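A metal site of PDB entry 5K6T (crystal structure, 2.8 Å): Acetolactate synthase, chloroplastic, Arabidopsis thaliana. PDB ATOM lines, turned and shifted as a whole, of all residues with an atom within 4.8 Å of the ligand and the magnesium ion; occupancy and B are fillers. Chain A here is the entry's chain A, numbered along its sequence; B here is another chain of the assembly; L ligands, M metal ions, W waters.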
ATOM      1  N   VAL A 400       8.025  18.468  16.330  1.00  0.00           N
ATOM      2  CA  VAL A 400       8.162  17.627  15.152  1.00  0.00           C
ATOM      3  C   VAL A 400       9.125  16.489  15.455  1.00  0.00           C
ATOM      4  O   VAL A 400      10.187  16.711  16.016  1.00  0.00           O
ATOM      5  CB  VAL A 400       8.674  18.441  13.946  1.00  0.00           C
ATOM      6  CG1 VAL A 400       9.059  17.520  12.799  1.00  0.00           C
ATOM      7  CG2 VAL A 400       7.624  19.453  13.491  1.00  0.00           C
ATOM      8  N   GLY A 401       8.725  15.273  15.093  1.00  0.00           N
ATOM      9  CA  GLY A 401       9.555  14.106  15.343  1.00  0.00           C
ATOM     10  C   GLY A 401       8.725  12.918  15.786  1.00  0.00           C
ATOM     11  O   GLY A 401       7.556  12.791  15.425  1.00  0.00           O
ATOM     12  N   GLN A 402       9.354  12.034  16.566  1.00  0.00           N
ATOM     13  CA  GLN A 402       8.679  10.836  17.049  1.00  0.00           C
ATOM     14  C   GLN A 402       7.485  11.168  17.944  1.00  0.00           C
ATOM     15  O   GLN A 402       6.412  10.573  17.800  1.00  0.00           O
ATOM     16  CB  GLN A 402       9.669   9.946  17.807  1.00  0.00           C
ATOM     17  CG  GLN A 402      10.698   9.274  16.934  1.00  0.00           C
ATOM     18  CD  GLN A 402      11.639   8.388  17.738  1.00  0.00           C
ATOM     19  OE1 GLN A 402      11.968   8.696  18.884  1.00  0.00           O
ATOM     20  NE2 GLN A 402      12.069   7.287  17.144  1.00  0.00           N
ATOM     21  N   HIS A 403       7.687  12.096  18.867  1.00  0.00           N
ATOM     22  CA  HIS A 403       6.639  12.486  19.803  1.00  0.00           C
ATOM     23  C   HIS A 403       5.441  13.081  19.072  1.00  0.00           C
ATOM     24  O   HIS A 403       4.300  12.971  19.529  1.00  0.00           O
ATOM     25  CB  HIS A 403       7.170  13.490  20.823  1.00  0.00           C
ATOM     26  CG  HIS A 403       7.420  14.862  20.262  1.00  0.00           C
ATOM     27  ND1 HIS A 403       8.564  15.174  19.554  1.00  0.00           N
ATOM     28  CD2 HIS A 403       6.668  15.988  20.294  1.00  0.00           C
ATOM     29  CE1 HIS A 403       8.499  16.439  19.180  1.00  0.00           C
ATOM     30  NE2 HIS A 403       7.372  16.954  19.609  1.00  0.00           N
ATOM     31  N   GLY A 426       6.969  20.947   8.722  1.00  0.00           N
ATOM     32  CA  GLY A 426       7.498  20.180   9.837  1.00  0.00           C
ATOM     33  C   GLY A 426       8.580  20.956  10.575  1.00  0.00           C
ATOM     34  O   GLY A 426       9.711  20.499  10.679  1.00  0.00           O
ATOM     35  N   ALA A 427       8.210  22.118  11.097  1.00  0.00           N
ATOM     36  CA  ALA A 427       9.155  23.005  11.763  1.00  0.00           C
ATOM     37  C   ALA A 427       9.259  22.721  13.262  1.00  0.00           C
ATOM     38  O   ALA A 427       8.254  22.776  13.981  1.00  0.00           O
ATOM     39  CB  ALA A 427       8.771  24.455  11.532  1.00  0.00           C
ATOM     40  N   MET A 428      10.467  22.438  13.737  1.00  0.00           N
ATOM     41  CA  MET A 428      10.714  22.301  15.165  1.00  0.00           C
ATOM     42  C   MET A 428      10.583  23.644  15.872  1.00  0.00           C
ATOM     43  O   MET A 428      10.738  24.695  15.255  1.00  0.00           O
ATOM     44  CB  MET A 428      12.100  21.701  15.413  1.00  0.00           C
ATOM     45  CG  MET A 428      12.244  20.258  14.967  1.00  0.00           C
ATOM     46  SD  MET A 428      13.921  19.643  15.144  1.00  0.00           S
ATOM     47  CE  MET A 428      14.151  19.756  16.916  1.00  0.00           C
ATOM     48  N   GLY A 452       9.159  17.504  22.240  1.00  0.00           N
ATOM     49  CA  GLY A 452      10.388  16.757  22.402  1.00  0.00           C
ATOM     50  C   GLY A 452      11.463  17.697  22.909  1.00  0.00           C
ATOM     51  O   GLY A 452      11.360  18.909  22.736  1.00  0.00           O
ATOM     52  N   ASP A 453      12.500  17.141  23.529  1.00  0.00           N
ATOM     53  CA  ASP A 453      13.537  17.947  24.164  1.00  0.00           C
ATOM     54  C   ASP A 453      14.344  18.761  23.144  1.00  0.00           C
ATOM     55  O   ASP A 453      14.896  19.799  23.478  1.00  0.00           O
ATOM     56  CB  ASP A 453      14.473  17.049  24.989  1.00  0.00           C
ATOM     57  CG  ASP A 453      15.003  15.875  24.188  1.00  0.00           C
ATOM     58  OD1 ASP A 453      14.243  15.305  23.373  1.00  0.00           O
ATOM     59  OD2 ASP A 453      16.185  15.517  24.376  1.00  0.00           O
ATOM     60  N   GLY A 454      14.391  18.276  21.910  1.00  0.00           N
ATOM     61  CA  GLY A 454      15.069  18.998  20.842  1.00  0.00           C
ATOM     62  C   GLY A 454      14.258  20.170  20.338  1.00  0.00           C
ATOM     63  O   GLY A 454      14.772  21.262  20.132  1.00  0.00           O
ATOM     64  N   SER A 455      12.966  19.937  20.136  1.00  0.00           N
ATOM     65  CA  SER A 455      12.062  20.975  19.629  1.00  0.00           C
ATOM     66  C   SER A 455      11.747  22.004  20.706  1.00  0.00           C
ATOM     67  O   SER A 455      11.595  23.193  20.408  1.00  0.00           O
ATOM     68  CB  SER A 455      10.764  20.338  19.105  1.00  0.00           C
ATOM     69  OG  SER A 455      11.025  19.406  18.076  1.00  0.00           O
ATOM     70  N   MET A 458      14.320  24.875  21.312  1.00  0.00           N
ATOM     71  CA  MET A 458      14.504  25.785  20.190  1.00  0.00           C
ATOM     72  C   MET A 458      13.828  27.134  20.409  1.00  0.00           C
ATOM     73  O   MET A 458      14.355  28.161  19.982  1.00  0.00           O
ATOM     74  CB  MET A 458      13.979  25.158  18.895  1.00  0.00           C
ATOM     75  CG  MET A 458      14.915  24.144  18.291  1.00  0.00           C
ATOM     76  SD  MET A 458      14.642  23.944  16.521  1.00  0.00           S
ATOM     77  CE  MET A 458      15.977  22.834  16.094  1.00  0.00           C
ATOM     78  N   LEU A 478       8.264  15.081  26.389  1.00  0.00           N
ATOM     79  CA  LEU A 478       8.755  13.720  26.212  1.00  0.00           C
ATOM     80  C   LEU A 478      10.265  13.764  25.944  1.00  0.00           C
ATOM     81  O   LEU A 478      10.699  14.061  24.828  1.00  0.00           O
ATOM     82  CB  LEU A 478       8.013  13.016  25.083  1.00  0.00           C
ATOM     83  CG  LEU A 478       6.483  12.976  25.242  1.00  0.00           C
ATOM     84  CD1 LEU A 478       5.825  12.242  24.084  1.00  0.00           C
ATOM     85  CD2 LEU A 478       6.100  12.334  26.568  1.00  0.00           C
ATOM     86  N   ASN A 480      13.805  12.149  25.526  1.00  0.00           N
ATOM     87  CA  ASN A 480      14.577  10.942  25.217  1.00  0.00           C
ATOM     88  C   ASN A 480      16.052  11.244  24.967  1.00  0.00           C
ATOM     89  O   ASN A 480      16.804  10.367  24.544  1.00  0.00           O
ATOM     90  CB  ASN A 480      13.970  10.233  23.992  1.00  0.00           C
ATOM     91  CG  ASN A 480      14.012  11.075  22.737  1.00  0.00           C
ATOM     92  OD1 ASN A 480      14.242  12.285  22.796  1.00  0.00           O
ATOM     93  ND2 ASN A 480      13.761  10.446  21.598  1.00  0.00           N
ATOM     94  N   GLN A 481      16.452  12.485  25.238  1.00  0.00           N
ATOM     95  CA  GLN A 481      17.835  12.930  25.147  1.00  0.00           C
ATOM     96  C   GLN A 481      18.424  12.837  23.736  1.00  0.00           C
ATOM     97  O   GLN A 481      19.638  12.942  23.561  1.00  0.00           O
ATOM     98  CB  GLN A 481      18.717  12.135  26.119  1.00  0.00           C
ATOM     99  CG  GLN A 481      18.374  12.341  27.580  1.00  0.00           C
ATOM    100  CD  GLN A 481      18.736  13.731  28.078  1.00  0.00           C
ATOM    101  OE1 GLN A 481      19.851  13.949  28.564  1.00  0.00           O
ATOM    102  NE2 GLN A 481      17.814  14.675  27.950  1.00  0.00           N
ATOM    103  N   HIS A 482      17.565  12.646  22.737  1.00  0.00           N
ATOM    104  CA  HIS A 482      18.030  12.507  21.365  1.00  0.00           C
ATOM    105  C   HIS A 482      17.103  13.204  20.373  1.00  0.00           C
ATOM    106  O   HIS A 482      15.993  13.605  20.723  1.00  0.00           O
ATOM    107  CB  HIS A 482      18.151  11.037  20.980  1.00  0.00           C
ATOM    108  CG  HIS A 482      19.263  10.303  21.673  1.00  0.00           C
ATOM    109  ND1 HIS A 482      19.151   9.831  22.966  1.00  0.00           N
ATOM    110  CD2 HIS A 482      20.508   9.955  21.256  1.00  0.00           C
ATOM    111  CE1 HIS A 482      20.274   9.225  23.307  1.00  0.00           C
ATOM    112  NE2 HIS A 482      21.113   9.292  22.295  1.00  0.00           N
ATOM    113  N   LEU A 483      17.583  13.344  19.143  1.00  0.00           N
ATOM    114  CA  LEU A 483      16.711  13.654  18.027  1.00  0.00           C
ATOM    115  C   LEU A 483      16.119  12.333  17.548  1.00  0.00           C
ATOM    116  O   LEU A 483      16.726  11.641  16.728  1.00  0.00           O
ATOM    117  CB  LEU A 483      17.470  14.382  16.916  1.00  0.00           C
ATOM    118  CG  LEU A 483      18.092  15.726  17.284  1.00  0.00           C
ATOM    119  CD1 LEU A 483      18.914  16.299  16.146  1.00  0.00           C
ATOM    120  CD2 LEU A 483      17.021  16.713  17.713  1.00  0.00           C
ATOM    121  N   GLY A 484      14.942  11.990  18.061  1.00  0.00           N
ATOM    122  CA  GLY A 484      14.350  10.683  17.881  1.00  0.00           C
ATOM    123  C   GLY A 484      14.182  10.155  16.467  1.00  0.00           C
ATOM    124  O   GLY A 484      14.654   9.067  16.145  1.00  0.00           O
ATOM    125  N   MET A 485      13.498  10.928  15.623  1.00  0.00           N
ATOM    126  CA  MET A 485      13.163  10.471  14.275  1.00  0.00           C
ATOM    127  C   MET A 485      14.394  10.260  13.392  1.00  0.00           C
ATOM    128  O   MET A 485      14.482   9.262  12.675  1.00  0.00           O
ATOM    129  CB  MET A 485      12.216  11.481  13.608  1.00  0.00           C
ATOM    130  CG  MET A 485      11.660  10.996  12.286  1.00  0.00           C
ATOM    131  SD  MET A 485      10.639   9.525  12.467  1.00  0.00           S
ATOM    132  CE  MET A 485       9.285  10.184  13.449  1.00  0.00           C
ATOM    133  N   VAL A 486      15.336  11.201  13.442  1.00  0.00           N
ATOM    134  CA  VAL A 486      16.582  11.078  12.697  1.00  0.00           C
ATOM    135  C   VAL A 486      17.362   9.868  13.177  1.00  0.00           C
ATOM    136  O   VAL A 486      17.929   9.112  12.388  1.00  0.00           O
ATOM    137  CB  VAL A 486      17.465  12.342  12.828  1.00  0.00           C
ATOM    138  CG1 VAL A 486      18.787  12.164  12.094  1.00  0.00           C
ATOM    139  CG2 VAL A 486      16.720  13.563  12.294  1.00  0.00           C
ATOM    140  N   LEU A 503      21.567  14.798  22.287  1.00  0.00           N
ATOM    141  CA  LEU A 503      21.349  16.174  22.740  1.00  0.00           C
ATOM    142  C   LEU A 503      21.864  16.443  24.147  1.00  0.00           C
ATOM    143  O   LEU A 503      21.843  17.587  24.618  1.00  0.00           O
ATOM    144  CB  LEU A 503      19.851  16.507  22.676  1.00  0.00           C
ATOM    145  CG  LEU A 503      19.208  16.506  21.294  1.00  0.00           C
ATOM    146  CD1 LEU A 503      17.705  16.662  21.417  1.00  0.00           C
ATOM    147  CD2 LEU A 503      19.794  17.604  20.419  1.00  0.00           C
ATOM    148  N   TYR B  33      23.238  21.269  11.895  1.00  0.00           N
ATOM    149  CA  TYR B  33      22.124  20.658  12.613  1.00  0.00           C
ATOM    150  C   TYR B  33      21.431  19.655  11.701  1.00  0.00           C
ATOM    151  O   TYR B  33      20.883  20.034  10.668  1.00  0.00           O
ATOM    152  CB  TYR B  33      21.142  21.720  13.101  1.00  0.00           C
ATOM    153  CG  TYR B  33      20.210  21.255  14.204  1.00  0.00           C
ATOM    154  CD1 TYR B  33      19.061  20.536  13.916  1.00  0.00           C
ATOM    155  CD2 TYR B  33      20.490  21.537  15.537  1.00  0.00           C
ATOM    156  CE1 TYR B  33      18.215  20.107  14.914  1.00  0.00           C
ATOM    157  CE2 TYR B  33      19.646  21.120  16.542  1.00  0.00           C
ATOM    158  CZ  TYR B  33      18.511  20.402  16.234  1.00  0.00           C
ATOM    159  OH  TYR B  33      17.667  19.985  17.239  1.00  0.00           O
ATOM    160  N   PRO B  34      21.444  18.371  12.078  1.00  0.00           N
ATOM    161  CA  PRO B  34      21.000  17.272  11.212  1.00  0.00           C
ATOM    162  C   PRO B  34      19.506  17.271  10.899  1.00  0.00           C
ATOM    163  O   PRO B  34      18.679  17.638  11.731  1.00  0.00           O
ATOM    164  CB  PRO B  34      21.376  16.024  12.007  1.00  0.00           C
ATOM    165  CG  PRO B  34      21.366  16.465  13.421  1.00  0.00           C
ATOM    166  CD  PRO B  34      21.877  17.881  13.398  1.00  0.00           C
ATOM    167  N   GLY B  35      19.178  16.866   9.681  1.00  0.00           N
ATOM    168  CA  GLY B  35      17.804  16.672   9.253  1.00  0.00           C
ATOM    169  C   GLY B  35      17.777  15.682   8.101  1.00  0.00           C
ATOM    170  O   GLY B  35      18.826  15.322   7.570  1.00  0.00           O
ATOM    171  N   GLY B  36      16.577  15.266   7.710  1.00  0.00           N
ATOM    172  CA  GLY B  36      16.403  14.243   6.689  1.00  0.00           C
ATOM    173  C   GLY B  36      17.124  14.485   5.380  1.00  0.00           C
ATOM    174  O   GLY B  36      17.765  13.578   4.834  1.00  0.00           O
ATOM    175  N   GLU B  59      19.299  26.366  14.190  1.00  0.00           N
ATOM    176  CA  GLU B  59      20.061  26.699  12.993  1.00  0.00           C
ATOM    177  C   GLU B  59      20.496  28.170  12.973  1.00  0.00           C
ATOM    178  O   GLU B  59      21.562  28.498  12.473  1.00  0.00           O
ATOM    179  CB  GLU B  59      19.264  26.380  11.727  1.00  0.00           C
ATOM    180  CG  GLU B  59      19.147  24.896  11.416  1.00  0.00           C
ATOM    181  CD  GLU B  59      17.900  24.264  12.016  1.00  0.00           C
ATOM    182  OE1 GLU B  59      17.161  24.964  12.727  1.00  0.00           O
ATOM    183  OE2 GLU B  59      17.652  23.066  11.744  1.00  0.00           O
ATOM    184  N   THR B  82      19.408  21.385   7.145  1.00  0.00           N
ATOM    185  CA  THR B  82      18.550  20.505   6.351  1.00  0.00           C
ATOM    186  C   THR B  82      17.584  21.346   5.530  1.00  0.00           C
ATOM    187  O   THR B  82      17.632  22.580   5.561  1.00  0.00           O
ATOM    188  CB  THR B  82      17.770  19.527   7.249  1.00  0.00           C
ATOM    189  OG1 THR B  82      17.137  18.537   6.449  1.00  0.00           O
ATOM    190  CG2 THR B  82      16.716  20.262   8.072  1.00  0.00           C
ATOM    191  N   PRO B  85      12.430  23.906   7.046  1.00  0.00           N
ATOM    192  CA  PRO B  85      12.526  24.713   8.255  1.00  0.00           C
ATOM    193  C   PRO B  85      13.976  24.956   8.690  1.00  0.00           C
ATOM    194  O   PRO B  85      14.276  25.971   9.317  1.00  0.00           O
ATOM    195  CB  PRO B  85      11.778  23.877   9.294  1.00  0.00           C
ATOM    196  CG  PRO B  85      11.883  22.482   8.796  1.00  0.00           C
ATOM    197  CD  PRO B  85      11.822  22.586   7.304  1.00  0.00           C
ATOM    198  N   GLY B  86      14.856  24.019   8.353  1.00  0.00           N
ATOM    199  CA  GLY B  86      16.274  24.180   8.635  1.00  0.00           C
ATOM    200  C   GLY B  86      16.854  25.323   7.825  1.00  0.00           C
ATOM    201  O   GLY B  86      17.539  26.196   8.357  1.00  0.00           O
ATOM    202  N   ASN B  89      15.620  28.857   8.688  1.00  0.00           N
ATOM    203  CA  ASN B  89      16.171  29.325   9.946  1.00  0.00           C
ATOM    204  C   ASN B  89      17.554  29.969   9.796  1.00  0.00           C
ATOM    205  O   ASN B  89      18.098  30.522  10.750  1.00  0.00           O
ATOM    206  CB  ASN B  89      16.241  28.181  10.955  1.00  0.00           C
ATOM    207  CG  ASN B  89      14.933  27.958  11.673  1.00  0.00           C
ATOM    208  OD1 ASN B  89      14.085  28.845  11.735  1.00  0.00           O
ATOM    209  ND2 ASN B  89      14.763  26.766  12.237  1.00  0.00           N
ATOM    210  N   GLN B 122       8.870  18.947   3.680  1.00  0.00           N
ATOM    211  CA  GLN B 122       9.969  19.809   4.116  1.00  0.00           C
ATOM    212  C   GLN B 122      10.696  20.475   2.937  1.00  0.00           C
ATOM    213  O   GLN B 122      11.923  20.493   2.896  1.00  0.00           O
ATOM    214  CB  GLN B 122      10.976  19.026   4.955  1.00  0.00           C
ATOM    215  CG  GLN B 122      10.397  18.470   6.240  1.00  0.00           C
ATOM    216  CD  GLN B 122      11.471  17.944   7.175  1.00  0.00           C
ATOM    217  OE1 GLN B 122      12.435  17.310   6.752  1.00  0.00           O
ATOM    218  NE2 GLN B 122      11.299  18.203   8.466  1.00  0.00           N
HETATM  219  N1  LIG L   1      15.371  21.292  12.064  1.00  0.00           N
HETATM  220  C1  LIG L   1      14.158  21.922  12.148  1.00  0.00           C
HETATM  221  C2  LIG L   1      14.072  23.408  12.579  1.00  0.00           C
HETATM  222  N2  LIG L   1      13.007  21.249  11.855  1.00  0.00           N
HETATM  223  C3  LIG L   1      13.070  19.946  11.476  1.00  0.00           C
HETATM  224  N3  LIG L   1      11.865  19.261  11.164  1.00  0.00           N
HETATM  225  C4  LIG L   1      14.286  19.299  11.391  1.00  0.00           C
HETATM  226  C5  LIG L   1      15.434  19.989  11.685  1.00  0.00           C
HETATM  227  C6  LIG L   1      14.350  17.852  10.960  1.00  0.00           C
HETATM  228  N4  LIG L   1      13.915  16.957  12.007  1.00  0.00           N
HETATM  229  C7  LIG L   1      12.771  16.101  11.972  1.00  0.00           C
HETATM  230  O1  LIG L   1      12.156  15.720  10.966  1.00  0.00           O
HETATM  231  S1  LIG L   1      12.428  15.742  13.441  1.00  0.00           S
HETATM  232  C8  LIG L   1      13.710  15.984  14.232  1.00  0.00           C
HETATM  233  C9  LIG L   1      14.617  16.715  13.381  1.00  0.00           C
HETATM  234  C10 LIG L   1      16.024  17.176  13.753  1.00  0.00           C
HETATM  235  C11 LIG L   1      14.003  15.544  15.671  1.00  0.00           C
HETATM  236  C12 LIG L   1      13.202  16.296  16.662  1.00  0.00           C
HETATM  237  O2  LIG L   1      13.714  16.002  17.971  1.00  0.00           O
HETATM  238  P1  LIG L   1      12.772  16.024  19.205  1.00  0.00           P
HETATM  239  O3  LIG L   1      11.553  15.051  18.949  1.00  0.00           O
HETATM  240  O4  LIG L   1      12.247  17.404  19.401  1.00  0.00           O
HETATM  241  O5  LIG L   1      13.527  15.593  20.423  1.00  0.00           O
HETATM  242  P2  LIG L   1      11.645  13.463  18.879  1.00  0.00           P
HETATM  243  O6  LIG L   1      11.921  13.044  17.465  1.00  0.00           O
HETATM  244  O7  LIG L   1      12.754  12.976  19.782  1.00  0.00           O
HETATM  245  O8  LIG L   1      10.319  12.886  19.347  1.00  0.00           O
HETATM  246 MG    MG M   1      14.101  13.999  21.631  1.00  0.00          MG
HETATM  247  O   HOH W   1      11.843  13.771  22.362  1.00  0.00           O
HETATM  248  O   HOH W   2      10.276  11.627  21.912  1.00  0.00           O
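Water W1 bridges the backbone carbonyl oxygen of Leu 478 (2.7 Å) and an oxygen (O8) of the ligand (3.5 Å).
O of Val 400 sits close to S1 of the ligand. The side-chain carboxylate of Glu 59 of chain B sits close to a nitrogen (N1) of the ligand (2.9 Å). CA of Gly 401 touches O6 of the ligand (3.4 Å). Gly 452 touches the ligand (CA to O4, 3.6 Å). Leu 483 touches the ligand (CD2 to O2, 3.4 Å). CG2 of Val 486 touches C9 of the ligand, 3.9 Å away. Tyr 33 of chain B touches the ligand. Pro 34 of chain B touches the ligand. Thr 82 of chain B touches the ligand. CG of Pro 85 of chain B touches N2 of the ligand, 3.5 Å away. Asn 89 of chain B touches the ligand (ND2 to C2, 3.4 Å). Hydrophobic or aromatic side chains within 4 Å of the ligand: Val 400, His 403, Met 428, Leu 483, Val 486, Tyr 33 of chain B and Pro 85 of chain B.
OD1 of Asn 480 binds the magnesium ion (2.1 Å). O5 of the ligand is bound to the magnesium ion, at 2.1 Å. The backbone carbonyl oxygen (O) of His 482 binds the magnesium ion, at 2.1 Å. OD1 of Asp 453 is bound to the magnesium ion, at 2.2 Å. Water W1 is bound to the magnesium ion (2.4 Å). The magnesium ion is bound by O7 of the ligand.
O4 of the ligand is in hydrogen-bond range of N of Ser 455 (2.7 Å). The side-chain hydroxyl (OG) of Ser 455 is in hydrogen-bond range of an oxygen (O4) of the ligand, 2.7 Å away. NE2 of Gln 122 of chain B lies close to N3 of the ligand (3.0 Å). O4 of the ligand sits at hydrogen-bond distance from N of Gly 454 (3.4 Å). An oxygen (O6) of the ligand sits at hydrogen-bond distance from the backbone NH (N) of Met 485 (3.2 Å). The backbone NH (N) of Gln 402 sits at hydrogen-bond distance from an oxygen (O6) of the ligand (2.9 Å). A nitrogen (N2) of the ligand lies close to the backbone NH (N) of Met 428, 3.4 Å away. N3 of the ligand lies within hydrogen-bond range of O of Gly 426 (2.5 Å). N of His 403 is in hydrogen-bond range of O8 of the ligand (2.8 Å). O8 of the ligand lies within hydrogen-bond range of ND1 of His 403 (2.9 Å). The backbone NH (N) of Gly 484 is in hydrogen-bond range of an oxygen (O6) of the ligand (3.3 Å).
Of the 31 residues printed, 3 come within 4 Å of the magnesium ion.
O of Val 400 lies within hydrogen-bond range of OG of Ser 455 (3.5 Å). NE2 of Gln 402 lies within hydrogen-bond range of O of Gly 484. The side-chain amide nitrogen of Asn 89 of chain B lies within hydrogen-bond range of the side-chain carboxylate of Glu 59 of chain B (3.0 Å). NE2 of His 403 sits at hydrogen-bond distance from N of Gly 452 (3.2 Å). N of Gln 481 sits close to OD2 of Asp 453, 3.2 Å away. The side-chain amide nitrogen (ND2) of Asn 89 of chain B is in hydrogen-bond range of the backbone carbonyl oxygen (O) of Pro 85 of chain B (3.1 Å).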
